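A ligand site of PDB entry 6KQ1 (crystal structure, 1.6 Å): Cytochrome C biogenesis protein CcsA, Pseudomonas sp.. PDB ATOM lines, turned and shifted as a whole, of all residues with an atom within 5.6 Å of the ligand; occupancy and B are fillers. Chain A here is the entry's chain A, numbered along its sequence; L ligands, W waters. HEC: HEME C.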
ATOM      1  N   PHE A   7     -26.536  16.075  16.638  1.00  0.00           N
ATOM      2  CA  PHE A   7     -27.389  17.136  16.132  1.00  0.00           C
ATOM      3  C   PHE A   7     -28.842  16.684  16.033  1.00  0.00           C
ATOM      4  O   PHE A   7     -29.763  17.483  16.250  1.00  0.00           O
ATOM      5  CB  PHE A   7     -26.900  17.611  14.756  1.00  0.00           C
ATOM      6  CG  PHE A   7     -27.810  18.626  14.114  1.00  0.00           C
ATOM      7  CD1 PHE A   7     -27.823  19.928  14.530  1.00  0.00           C
ATOM      8  CD2 PHE A   7     -28.679  18.242  13.109  1.00  0.00           C
ATOM      9  CE1 PHE A   7     -28.686  20.855  13.940  1.00  0.00           C
ATOM     10  CE2 PHE A   7     -29.529  19.159  12.521  1.00  0.00           C
ATOM     11  CZ  PHE A   7     -29.523  20.468  12.936  1.00  0.00           C
ATOM     12  N   LYS A  10     -30.194  15.260  19.980  1.00  0.00           N
ATOM     13  CA  LYS A  10     -30.400  16.371  20.920  1.00  0.00           C
ATOM     14  C   LYS A  10     -31.432  17.318  20.320  1.00  0.00           C
ATOM     15  O   LYS A  10     -31.891  17.073  19.195  1.00  0.00           O
ATOM     16  CB  LYS A  10     -29.043  17.033  21.196  1.00  0.00           C
ATOM     17  CG  LYS A  10     -28.002  16.091  21.796  1.00  0.00           C
ATOM     18  CD  LYS A  10     -28.441  15.530  23.151  1.00  0.00           C
ATOM     19  CE  LYS A  10     -27.372  14.630  23.757  1.00  0.00           C
ATOM     20  NZ  LYS A  10     -27.753  14.213  25.150  1.00  0.00           N
ATOM     21  N   PRO A  11     -31.863  18.383  21.004  1.00  0.00           N
ATOM     22  CA  PRO A  11     -32.958  19.193  20.458  1.00  0.00           C
ATOM     23  C   PRO A  11     -32.565  20.202  19.395  1.00  0.00           C
ATOM     24  O   PRO A  11     -33.403  21.042  19.036  1.00  0.00           O
ATOM     25  CB  PRO A  11     -33.508  19.925  21.699  1.00  0.00           C
ATOM     26  CG  PRO A  11     -32.459  19.869  22.697  1.00  0.00           C
ATOM     27  CD  PRO A  11     -31.605  18.683  22.422  1.00  0.00           C
ATOM     28  N   CYS A  12     -31.356  20.106  18.832  1.00  0.00           N
ATOM     29  CA  CYS A  12     -30.815  21.197  17.998  1.00  0.00           C
ATOM     30  C   CYS A  12     -31.707  21.521  16.806  1.00  0.00           C
ATOM     31  O   CYS A  12     -31.792  22.685  16.393  1.00  0.00           O
ATOM     32  CB  CYS A  12     -29.422  20.835  17.490  1.00  0.00           C
ATOM     33  SG  CYS A  12     -28.368  20.128  18.730  1.00  0.00           S
ATOM     34  N   ALA A  14     -34.776  21.686  16.415  1.00  0.00           N
ATOM     35  CA  ALA A  14     -35.917  22.541  16.673  1.00  0.00           C
ATOM     36  C   ALA A  14     -35.617  23.976  16.294  1.00  0.00           C
ATOM     37  O   ALA A  14     -36.539  24.735  15.994  1.00  0.00           O
ATOM     38  CB  ALA A  14     -36.310  22.471  18.147  1.00  0.00           C
ATOM     39  N   CYS A  15     -34.339  24.359  16.291  1.00  0.00           N
ATOM     40  CA  CYS A  15     -33.932  25.747  16.143  1.00  0.00           C
ATOM     41  C   CYS A  15     -32.897  25.975  15.069  1.00  0.00           C
ATOM     42  O   CYS A  15     -32.689  27.131  14.685  1.00  0.00           O
ATOM     43  CB  CYS A  15     -33.373  26.286  17.466  1.00  0.00           C
ATOM     44  SG  CYS A  15     -34.597  26.363  18.794  1.00  0.00           S
ATOM     45  N   HIS A  16     -32.224  24.928  14.582  1.00  0.00           N
ATOM     46  CA  HIS A  16     -31.133  25.084  13.629  1.00  0.00           C
ATOM     47  C   HIS A  16     -31.343  24.162  12.433  1.00  0.00           C
ATOM     48  O   HIS A  16     -31.833  23.031  12.563  1.00  0.00           O
ATOM     49  CB  HIS A  16     -29.792  24.726  14.221  1.00  0.00           C
ATOM     50  CG  HIS A  16     -29.298  25.685  15.244  1.00  0.00           C
ATOM     51  ND1 HIS A  16     -28.723  26.893  14.906  1.00  0.00           N
ATOM     52  CD2 HIS A  16     -29.244  25.590  16.591  1.00  0.00           C
ATOM     53  CE1 HIS A  16     -28.355  27.507  16.014  1.00  0.00           C
ATOM     54  NE2 HIS A  16     -28.647  26.744  17.046  1.00  0.00           N
ATOM     55  N   VAL A  23     -34.518  29.486  13.873  1.00  0.00           N
ATOM     56  CA  VAL A  23     -34.423  30.342  15.060  1.00  0.00           C
ATOM     57  C   VAL A  23     -32.984  30.820  15.254  1.00  0.00           C
ATOM     58  O   VAL A  23     -32.725  32.020  15.386  1.00  0.00           O
ATOM     59  CB  VAL A  23     -34.896  29.558  16.306  1.00  0.00           C
ATOM     60  CG1 VAL A  23     -34.912  30.461  17.521  1.00  0.00           C
ATOM     61  CG2 VAL A  23     -36.279  28.917  16.076  1.00  0.00           C
ATOM     62  N   GLY A  24     -32.042  29.882  15.235  1.00  0.00           N
ATOM     63  CA  GLY A  24     -30.644  30.192  15.345  1.00  0.00           C
ATOM     64  C   GLY A  24     -30.009  30.233  13.976  1.00  0.00           C
ATOM     65  O   GLY A  24     -30.619  29.872  12.981  1.00  0.00           O
ATOM     66  N   PRO A  25     -28.767  30.708  13.920  1.00  0.00           N
ATOM     67  CA  PRO A  25     -28.056  30.762  12.635  1.00  0.00           C
ATOM     68  C   PRO A  25     -27.891  29.382  12.024  1.00  0.00           C
ATOM     69  O   PRO A  25     -27.749  28.383  12.724  1.00  0.00           O
ATOM     70  CB  PRO A  25     -26.700  31.359  13.016  1.00  0.00           C
ATOM     71  CG  PRO A  25     -26.530  30.955  14.448  1.00  0.00           C
ATOM     72  CD  PRO A  25     -27.902  31.095  15.039  1.00  0.00           C
ATOM     73  N   LEU A  27     -25.978  26.370  10.655  1.00  0.00           N
ATOM     74  CA  LEU A  27     -24.713  25.892  11.205  1.00  0.00           C
ATOM     75  C   LEU A  27     -23.560  26.139  10.242  1.00  0.00           C
ATOM     76  O   LEU A  27     -22.423  26.352  10.687  1.00  0.00           O
ATOM     77  CB  LEU A  27     -24.843  24.429  11.588  1.00  0.00           C
ATOM     78  CG  LEU A  27     -25.824  24.246  12.761  1.00  0.00           C
ATOM     79  CD1 LEU A  27     -25.868  22.802  13.241  1.00  0.00           C
ATOM     80  CD2 LEU A  27     -25.570  25.215  13.913  1.00  0.00           C
ATOM     81  N   VAL A  30     -22.371  29.587  10.994  1.00  0.00           N
ATOM     82  CA  VAL A  30     -21.525  29.629  12.190  1.00  0.00           C
ATOM     83  C   VAL A  30     -20.100  29.236  11.825  1.00  0.00           C
ATOM     84  O   VAL A  30     -19.135  29.889  12.226  1.00  0.00           O
ATOM     85  CB  VAL A  30     -22.106  28.734  13.298  1.00  0.00           C
ATOM     86  CG1 VAL A  30     -21.188  28.700  14.522  1.00  0.00           C
ATOM     87  CG2 VAL A  30     -23.492  29.204  13.714  1.00  0.00           C
ATOM     88  N   TYR A  34     -16.665  31.758  12.233  1.00  0.00           N
ATOM     89  CA  TYR A  34     -15.591  31.439  13.164  1.00  0.00           C
ATOM     90  C   TYR A  34     -14.407  30.798  12.479  1.00  0.00           C
ATOM     91  O   TYR A  34     -13.445  30.414  13.156  1.00  0.00           O
ATOM     92  CB  TYR A  34     -16.119  30.550  14.285  1.00  0.00           C
ATOM     93  CG  TYR A  34     -17.064  31.284  15.204  1.00  0.00           C
ATOM     94  CD1 TYR A  34     -16.583  32.224  16.109  1.00  0.00           C
ATOM     95  CD2 TYR A  34     -18.436  31.063  15.157  1.00  0.00           C
ATOM     96  CE1 TYR A  34     -17.428  32.904  16.951  1.00  0.00           C
ATOM     97  CE2 TYR A  34     -19.301  31.766  15.995  1.00  0.00           C
ATOM     98  CZ  TYR A  34     -18.780  32.682  16.897  1.00  0.00           C
ATOM     99  OH  TYR A  34     -19.604  33.396  17.754  1.00  0.00           O
ATOM    100  N   LEU A  43     -14.926  27.941  22.679  1.00  0.00           N
ATOM    101  CA  LEU A  43     -15.960  28.957  22.850  1.00  0.00           C
ATOM    102  C   LEU A  43     -17.338  28.423  22.479  1.00  0.00           C
ATOM    103  O   LEU A  43     -18.302  28.554  23.235  1.00  0.00           O
ATOM    104  CB  LEU A  43     -15.617  30.180  22.014  1.00  0.00           C
ATOM    105  CG  LEU A  43     -16.545  31.375  22.194  1.00  0.00           C
ATOM    106  CD1 LEU A  43     -16.503  31.865  23.628  1.00  0.00           C
ATOM    107  CD2 LEU A  43     -16.204  32.490  21.227  1.00  0.00           C
ATOM    108  N   LEU A  44     -17.443  27.802  21.299  1.00  0.00           N
ATOM    109  CA  LEU A  44     -18.732  27.303  20.849  1.00  0.00           C
ATOM    110  C   LEU A  44     -19.208  26.160  21.729  1.00  0.00           C
ATOM    111  O   LEU A  44     -20.403  26.041  22.000  1.00  0.00           O
ATOM    112  CB  LEU A  44     -18.649  26.849  19.401  1.00  0.00           C
ATOM    113  CG  LEU A  44     -18.390  27.908  18.336  1.00  0.00           C
ATOM    114  CD1 LEU A  44     -18.328  27.207  17.005  1.00  0.00           C
ATOM    115  CD2 LEU A  44     -19.471  28.952  18.294  1.00  0.00           C
ATOM    116  N   HIS A  47     -20.874  27.593  24.608  1.00  0.00           N
ATOM    117  CA  HIS A  47     -22.141  28.201  24.229  1.00  0.00           C
ATOM    118  C   HIS A  47     -23.210  27.150  23.958  1.00  0.00           C
ATOM    119  O   HIS A  47     -24.383  27.345  24.315  1.00  0.00           O
ATOM    120  CB  HIS A  47     -21.936  29.081  23.003  1.00  0.00           C
ATOM    121  CG  HIS A  47     -21.223  30.360  23.320  1.00  0.00           C
ATOM    122  ND1 HIS A  47     -20.873  31.271  22.353  1.00  0.00           N
ATOM    123  CD2 HIS A  47     -20.830  30.888  24.501  1.00  0.00           C
ATOM    124  CE1 HIS A  47     -20.267  32.304  22.924  1.00  0.00           C
ATOM    125  NE2 HIS A  47     -20.238  32.092  24.228  1.00  0.00           N
ATOM    126  N   ILE A  48     -22.832  26.032  23.306  1.00  0.00           N
ATOM    127  CA  ILE A  48     -23.804  24.977  23.028  1.00  0.00           C
ATOM    128  C   ILE A  48     -24.337  24.403  24.329  1.00  0.00           C
ATOM    129  O   ILE A  48     -25.555  24.242  24.507  1.00  0.00           O
ATOM    130  CB  ILE A  48     -23.161  23.878  22.148  1.00  0.00           C
ATOM    131  CG1 ILE A  48     -22.857  24.418  20.747  1.00  0.00           C
ATOM    132  CG2 ILE A  48     -24.062  22.663  22.065  1.00  0.00           C
ATOM    133  CD1 ILE A  48     -21.915  23.536  19.941  1.00  0.00           C
ATOM    134  N   THR A  52     -26.216  30.995  25.079  1.00  0.00           N
ATOM    135  CA  THR A  52     -25.626  32.282  24.762  1.00  0.00           C
ATOM    136  C   THR A  52     -26.682  33.139  24.099  1.00  0.00           C
ATOM    137  O   THR A  52     -27.773  32.673  23.772  1.00  0.00           O
ATOM    138  CB  THR A  52     -24.382  32.117  23.874  1.00  0.00           C
ATOM    139  OG1 THR A  52     -23.717  33.386  23.768  1.00  0.00           O
ATOM    140  CG2 THR A  52     -24.753  31.637  22.497  1.00  0.00           C
ATOM    141  N   GLN A  53     -26.376  34.417  23.936  1.00  0.00           N
ATOM    142  CA  GLN A  53     -27.292  35.364  23.313  1.00  0.00           C
ATOM    143  C   GLN A  53     -26.484  36.548  22.828  1.00  0.00           C
ATOM    144  O   GLN A  53     -25.392  36.808  23.329  1.00  0.00           O
ATOM    145  CB  GLN A  53     -28.391  35.799  24.295  1.00  0.00           C
ATOM    146  CG  GLN A  53     -29.399  36.776  23.732  1.00  0.00           C
ATOM    147  CD  GLN A  53     -29.629  37.953  24.661  1.00  0.00           C
ATOM    148  OE1 GLN A  53     -29.804  37.786  25.871  1.00  0.00           O
ATOM    149  NE2 GLN A  53     -29.624  39.160  24.088  1.00  0.00           N
ATOM    150  N   GLY A  54     -26.992  37.228  21.799  1.00  0.00           N
ATOM    151  CA  GLY A  54     -26.432  38.498  21.407  1.00  0.00           C
ATOM    152  C   GLY A  54     -25.249  38.431  20.465  1.00  0.00           C
ATOM    153  O   GLY A  54     -24.682  39.488  20.154  1.00  0.00           O
ATOM    154  N   ASN A  55     -24.839  37.235  20.035  1.00  0.00           N
ATOM    155  CA  ASN A  55     -23.832  37.075  18.989  1.00  0.00           C
ATOM    156  C   ASN A  55     -24.437  37.125  17.595  1.00  0.00           C
ATOM    157  O   ASN A  55     -23.737  37.446  16.621  1.00  0.00           O
ATOM    158  CB  ASN A  55     -23.094  35.726  19.111  1.00  0.00           C
ATOM    159  CG  ASN A  55     -22.569  35.456  20.509  1.00  0.00           C
ATOM    160  OD1 ASN A  55     -23.094  34.596  21.230  1.00  0.00           O
ATOM    161  ND2 ASN A  55     -21.516  36.154  20.888  1.00  0.00           N
ATOM    162  N   TRP A  56     -25.714  36.773  17.471  1.00  0.00           N
ATOM    163  CA  TRP A  56     -26.427  36.760  16.204  1.00  0.00           C
ATOM    164  C   TRP A  56     -27.712  37.556  16.222  1.00  0.00           C
ATOM    165  O   TRP A  56     -28.240  37.868  15.146  1.00  0.00           O
ATOM    166  CB  TRP A  56     -26.759  35.320  15.779  1.00  0.00           C
ATOM    167  CG  TRP A  56     -25.526  34.495  15.622  1.00  0.00           C
ATOM    168  CD1 TRP A  56     -24.849  33.838  16.602  1.00  0.00           C
ATOM    169  CD2 TRP A  56     -24.823  34.261  14.411  1.00  0.00           C
ATOM    170  NE1 TRP A  56     -23.749  33.195  16.076  1.00  0.00           N
ATOM    171  CE2 TRP A  56     -23.724  33.425  14.718  1.00  0.00           C
ATOM    172  CE3 TRP A  56     -25.021  34.643  13.084  1.00  0.00           C
ATOM    173  CZ2 TRP A  56     -22.828  32.994  13.751  1.00  0.00           C
ATOM    174  CZ3 TRP A  56     -24.132  34.204  12.126  1.00  0.00           C
ATOM    175  CH2 TRP A  56     -23.047  33.382  12.459  1.00  0.00           C
ATOM    176  N   GLY A  57     -28.237  37.878  17.387  1.00  0.00           N
ATOM    177  CA  GLY A  57     -29.485  38.587  17.485  1.00  0.00           C
ATOM    178  C   GLY A  57     -29.976  38.572  18.913  1.00  0.00           C
ATOM    179  O   GLY A  57     -29.280  38.118  19.835  1.00  0.00           O
ATOM    180  N   PRO A  58     -31.203  39.064  19.123  1.00  0.00           N
ATOM    181  CA  PRO A  58     -31.701  39.175  20.500  1.00  0.00           C
ATOM    182  C   PRO A  58     -32.283  37.880  21.055  1.00  0.00           C
ATOM    183  O   PRO A  58     -32.442  37.790  22.273  1.00  0.00           O
ATOM    184  CB  PRO A  58     -32.790  40.254  20.371  1.00  0.00           C
ATOM    185  CG  PRO A  58     -33.280  40.128  18.952  1.00  0.00           C
ATOM    186  CD  PRO A  58     -32.130  39.609  18.122  1.00  0.00           C
ATOM    187  N   ILE A  59     -32.587  36.902  20.207  1.00  0.00           N
ATOM    188  CA  ILE A  59     -33.180  35.648  20.669  1.00  0.00           C
ATOM    189  C   ILE A  59     -32.071  34.785  21.275  1.00  0.00           C
ATOM    190  O   ILE A  59     -31.031  34.578  20.619  1.00  0.00           O
ATOM    191  CB  ILE A  59     -33.865  34.929  19.503  1.00  0.00           C
ATOM    192  CG1 ILE A  59     -35.021  35.787  18.969  1.00  0.00           C
ATOM    193  CG2 ILE A  59     -34.344  33.520  19.892  1.00  0.00           C
ATOM    194  CD1 ILE A  59     -35.664  35.228  17.708  1.00  0.00           C
ATOM    195  N   PRO A  60     -32.217  34.304  22.507  1.00  0.00           N
ATOM    196  CA  PRO A  60     -31.170  33.498  23.132  1.00  0.00           C
ATOM    197  C   PRO A  60     -31.248  32.033  22.724  1.00  0.00           C
ATOM    198  O   PRO A  60     -32.312  31.497  22.417  1.00  0.00           O
ATOM    199  CB  PRO A  60     -31.472  33.648  24.622  1.00  0.00           C
ATOM    200  CG  PRO A  60     -32.974  33.744  24.647  1.00  0.00           C
ATOM    201  CD  PRO A  60     -33.334  34.572  23.447  1.00  0.00           C
ATOM    202  N   MET A  61     -30.081  31.375  22.782  1.00  0.00           N
ATOM    203  CA  MET A  61     -30.038  29.926  22.803  1.00  0.00           C
ATOM    204  C   MET A  61     -30.006  29.466  24.253  1.00  0.00           C
ATOM    205  O   MET A  61     -29.031  29.764  24.949  1.00  0.00           O
ATOM    206  CB  MET A  61     -28.823  29.395  22.068  1.00  0.00           C
ATOM    207  CG  MET A  61     -28.665  27.864  22.247  1.00  0.00           C
ATOM    208  SD  MET A  61     -27.436  26.983  21.282  1.00  0.00           S
ATOM    209  CE  MET A  61     -25.967  28.002  21.485  1.00  0.00           C
ATOM    210  N   PRO A  62     -31.016  28.758  24.739  1.00  0.00           N
ATOM    211  CA  PRO A  62     -30.980  28.270  26.107  1.00  0.00           C
ATOM    212  C   PRO A  62     -29.898  27.216  26.267  1.00  0.00           C
ATOM    213  O   PRO A  62     -29.410  26.672  25.264  1.00  0.00           O
ATOM    214  CB  PRO A  62     -32.377  27.664  26.310  1.00  0.00           C
ATOM    215  CG  PRO A  62     -33.215  28.273  25.225  1.00  0.00           C
ATOM    216  CD  PRO A  62     -32.273  28.391  24.070  1.00  0.00           C
ATOM    217  N   ASN A  64     -28.334  23.581  26.602  1.00  0.00           N
ATOM    218  CA  ASN A  64     -28.740  22.338  25.983  1.00  0.00           C
ATOM    219  C   ASN A  64     -28.376  21.137  26.841  1.00  0.00           C
ATOM    220  O   ASN A  64     -27.404  21.184  27.597  1.00  0.00           O
ATOM    221  CB  ASN A  64     -28.070  22.194  24.619  1.00  0.00           C
ATOM    222  CG  ASN A  64     -28.743  23.032  23.570  1.00  0.00           C
ATOM    223  OD1 ASN A  64     -29.876  22.762  23.185  1.00  0.00           O
ATOM    224  ND2 ASN A  64     -28.042  24.074  23.110  1.00  0.00           N
ATOM    225  N   VAL A  66     -26.586  18.525  26.995  1.00  0.00           N
ATOM    226  CA  VAL A  66     -25.392  17.881  26.439  1.00  0.00           C
ATOM    227  C   VAL A  66     -24.304  17.842  27.498  1.00  0.00           C
ATOM    228  O   VAL A  66     -24.185  18.743  28.339  1.00  0.00           O
ATOM    229  CB  VAL A  66     -24.849  18.614  25.189  1.00  0.00           C
ATOM    230  CG1 VAL A  66     -25.854  18.498  24.078  1.00  0.00           C
ATOM    231  CG2 VAL A  66     -24.546  20.088  25.521  1.00  0.00           C
ATOM    232  N   LEU A  74     -19.881  18.397  19.126  1.00  0.00           N
ATOM    233  CA  LEU A  74     -20.757  19.226  18.317  1.00  0.00           C
ATOM    234  C   LEU A  74     -20.051  20.483  17.811  1.00  0.00           C
ATOM    235  O   LEU A  74     -20.227  20.865  16.649  1.00  0.00           O
ATOM    236  CB  LEU A  74     -22.000  19.614  19.128  1.00  0.00           C
ATOM    237  CG  LEU A  74     -23.028  18.490  19.216  1.00  0.00           C
ATOM    238  CD1 LEU A  74     -23.912  18.791  20.451  1.00  0.00           C
ATOM    239  CD2 LEU A  74     -23.874  18.406  17.955  1.00  0.00           C
ATOM    240  N   VAL A  78     -19.626  21.402  13.989  1.00  0.00           N
ATOM    241  CA  VAL A  78     -20.135  22.646  13.411  1.00  0.00           C
ATOM    242  C   VAL A  78     -19.022  23.376  12.662  1.00  0.00           C
ATOM    243  O   VAL A  78     -19.208  23.850  11.527  1.00  0.00           O
ATOM    244  CB  VAL A  78     -20.766  23.519  14.498  1.00  0.00           C
ATOM    245  CG1 VAL A  78     -20.951  24.944  14.001  1.00  0.00           C
ATOM    246  CG2 VAL A  78     -22.130  22.951  14.924  1.00  0.00           C
HETATM  247 FE   HEC L   1     -28.167  26.953  18.904  1.00  0.00          FE
HETATM  248  CHA HEC L   1     -26.431  29.853  18.423  1.00  0.00           C
HETATM  249  CHB HEC L   1     -25.438  25.149  18.043  1.00  0.00           C
HETATM  250  CHC HEC L   1     -29.701  24.135  20.101  1.00  0.00           C
HETATM  251  CHD HEC L   1     -31.063  28.645  19.066  1.00  0.00           C
HETATM  252  NA  HEC L   1     -26.294  27.412  18.352  1.00  0.00           N
HETATM  253  C1A HEC L   1     -25.756  28.672  18.205  1.00  0.00           C
HETATM  254  C2A HEC L   1     -24.371  28.531  17.794  1.00  0.00           C
HETATM  255  C3A HEC L   1     -24.101  27.228  17.694  1.00  0.00           C
HETATM  256  C4A HEC L   1     -25.301  26.515  18.037  1.00  0.00           C
HETATM  257  CMA HEC L   1     -22.786  26.543  17.296  1.00  0.00           C
HETATM  258  CAA HEC L   1     -23.444  29.727  17.550  1.00  0.00           C
HETATM  259  CBA HEC L   1     -22.944  30.316  18.885  1.00  0.00           C
HETATM  260  CGA HEC L   1     -21.934  31.444  18.732  1.00  0.00           C
HETATM  261  O1A HEC L   1     -22.015  32.119  17.682  1.00  0.00           O
HETATM  262  O2A HEC L   1     -21.175  31.597  19.707  1.00  0.00           O
HETATM  263  NB  HEC L   1     -27.666  25.021  19.039  1.00  0.00           N
HETATM  264  C1B HEC L   1     -26.474  24.470  18.618  1.00  0.00           C
HETATM  265  C2B HEC L   1     -26.503  23.061  18.883  1.00  0.00           C
HETATM  266  C3B HEC L   1     -27.685  22.786  19.455  1.00  0.00           C
HETATM  267  C4B HEC L   1     -28.428  24.014  19.564  1.00  0.00           C
HETATM  268  CMB HEC L   1     -25.334  22.110  18.541  1.00  0.00           C
HETATM  269  CAB HEC L   1     -28.159  21.380  19.930  1.00  0.00           C
HETATM  270  CBB HEC L   1     -27.365  20.918  20.989  1.00  0.00           C
HETATM  271  NC  HEC L   1     -30.025  26.487  19.471  1.00  0.00           N
HETATM  272  C1C HEC L   1     -30.463  25.277  19.939  1.00  0.00           C
HETATM  273  C2C HEC L   1     -31.879  25.365  20.252  1.00  0.00           C
HETATM  274  C3C HEC L   1     -32.254  26.619  19.959  1.00  0.00           C
HETATM  275  C4C HEC L   1     -31.118  27.337  19.478  1.00  0.00           C
HETATM  276  CMC HEC L   1     -32.700  24.172  20.797  1.00  0.00           C
HETATM  277  CAC HEC L   1     -33.690  27.263  20.085  1.00  0.00           C
HETATM  278  CBC HEC L   1     -34.360  27.042  21.249  1.00  0.00           C
HETATM  279  ND  HEC L   1     -28.642  28.900  18.758  1.00  0.00           N
HETATM  280  C1D HEC L   1     -29.929  29.389  18.861  1.00  0.00           C
HETATM  281  C2D HEC L   1     -29.854  30.814  18.715  1.00  0.00           C
HETATM  282  C3D HEC L   1     -28.586  31.160  18.531  1.00  0.00           C
HETATM  283  C4D HEC L   1     -27.793  29.940  18.571  1.00  0.00           C
HETATM  284  CMD HEC L   1     -31.119  31.709  18.779  1.00  0.00           C
HETATM  285  CAD HEC L   1     -28.005  32.563  18.365  1.00  0.00           C
HETATM  286  CBD HEC L   1     -27.683  33.233  19.708  1.00  0.00           C
HETATM  287  CGD HEC L   1     -27.004  34.559  19.635  1.00  0.00           C
HETATM  288  O1D HEC L   1     -27.601  35.399  18.909  1.00  0.00           O
HETATM  289  O2D HEC L   1     -25.868  34.666  20.136  1.00  0.00           O
HETATM  290  O   HOH W   1     -30.177  35.254  18.033  1.00  0.00           O
HETATM  291  O   HOH W   2     -31.221  25.286  23.613  1.00  0.00           O
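A carbon (CAB) of the ligand is covalently linked to the side-chain sulfur of Cys 12 (1.7 Å).
N of Gly 54 lies within hydrogen-bond range of O2D of the ligand, at 3.3 Å.
The side-chain sulfur (SD) of Met 61 is bound to an iron atom (FE) of the ligand (2.5 Å).
A carbon (CAC) of the ligand is covalently linked to the side-chain sulfur (SG) of Cys 15 (1.8 Å).
A ring nitrogen (NE2) of His 16 is bound to an iron atom (FE) of the ligand (1.9 Å).
N of Asn 55 is in hydrogen-bond range of O2D of the ligand.
An oxygen (O1A) of the ligand is in hydrogen-bond range of the indole nitrogen (NE1) of Trp 56, 2.6 Å away.
A ring nitrogen (ND1) of His 47 lies within hydrogen-bond range of an oxygen (O2A) of the ligand (2.7 Å).
The side-chain amide oxygen (OD1) of Asn 55 sits close to an oxygen (O2D) of the ligand, at 3.0 Å.
N of Trp 56 sits at hydrogen-bond distance from O1D of the ligand, 2.7 Å away.
The side-chain hydroxyl (OH) of Tyr 34 sits at hydrogen-bond distance from an oxygen (O1A) of the ligand.
The backbone NH (N) of Gly 57 sits at hydrogen-bond distance from an oxygen (O1D) of the ligand, 3.0 Å away.
The backbone NH (N) of Met 61 is in hydrogen-bond range of the backbone carbonyl oxygen (O) of Thr 52, at 2.8 Å.
O of Pro 25 is in hydrogen-bond range of ND1 of His 16 (2.8 Å).
The backbone NH of Gly 24 sits at hydrogen-bond distance from the backbone carbonyl oxygen of Cys 15, at 2.9 Å.
The side-chain amide nitrogen of Asn 64 sits close to the side-chain sulfur of Met 61, at 3.5 Å.
The side-chain hydroxyl (OG1) of Thr 52 sits at hydrogen-bond distance from the side-chain amide oxygen (OD1) of Asn 55 (2.9 Å).
ND2 of Asn 64 is in hydrogen-bond range of O of Ile 48 (2.9 Å).
N of Val 23 sits at hydrogen-bond distance from O of Cys 15 (3.1 Å).
Pro 11 touches the ligand (O to CMC, 3.7 Å).
Val 23 touches the ligand (O to CMD, 3.8 Å).
Gly 24 touches the ligand (CA to C2D, 3.5 Å).
Pro 25 touches the ligand.
CG1 of Val 30 touches CMA of the ligand, 3.9 Å away.
CD2 of Leu 44 touches O2A of the ligand, 3.4 Å away.
Ile 48 touches the ligand (CG2 to CMB, 3.8 Å).
CG2 of Thr 52 touches O2D of the ligand, at 3.999 Å.
Gln 53 touches the ligand.
Ile 59 touches the ligand (O to CMD, 3.4 Å).
Pro 60 touches the ligand (O to CMD, 3.8 Å).
CD of Pro 62 touches CBC of the ligand, 3.8 Å away.
Asn 64 touches the ligand.
Hydrophobic or aromatic side chains within 4 Å of the ligand: His 16, Pro 25, Val 30, Tyr 34, Leu 44, His 47, Ile 48, Trp 56, Ile 59, Met 61 and Pro 62.
23 residues have an atom within 4 Å of the ligand: Pro 11, Cys 12, Cys 15, His 16, Val 23, Gly 24, Pro 25, Val 30, Tyr 34, Leu 44, His 47, Ile 48, Thr 52, Gln 53, Gly 54, Asn 55, Trp 56, Gly 57, Ile 59, Pro 60, Met 61, Pro 62 and Asn 64.
The nearest printed residue that does not touch the ligand is Leu 74 (4.02 Å).
Water W1 lies within hydrogen-bond range of an oxygen (O1D) of the ligand (2.7 Å), the backbone carbonyl oxygen of Ile 59 (2.8 Å) and the backbone NH of Gly 57 (3.3 Å).
Water W2 bridges O of Pro 62 and OD1 of Asn 64.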
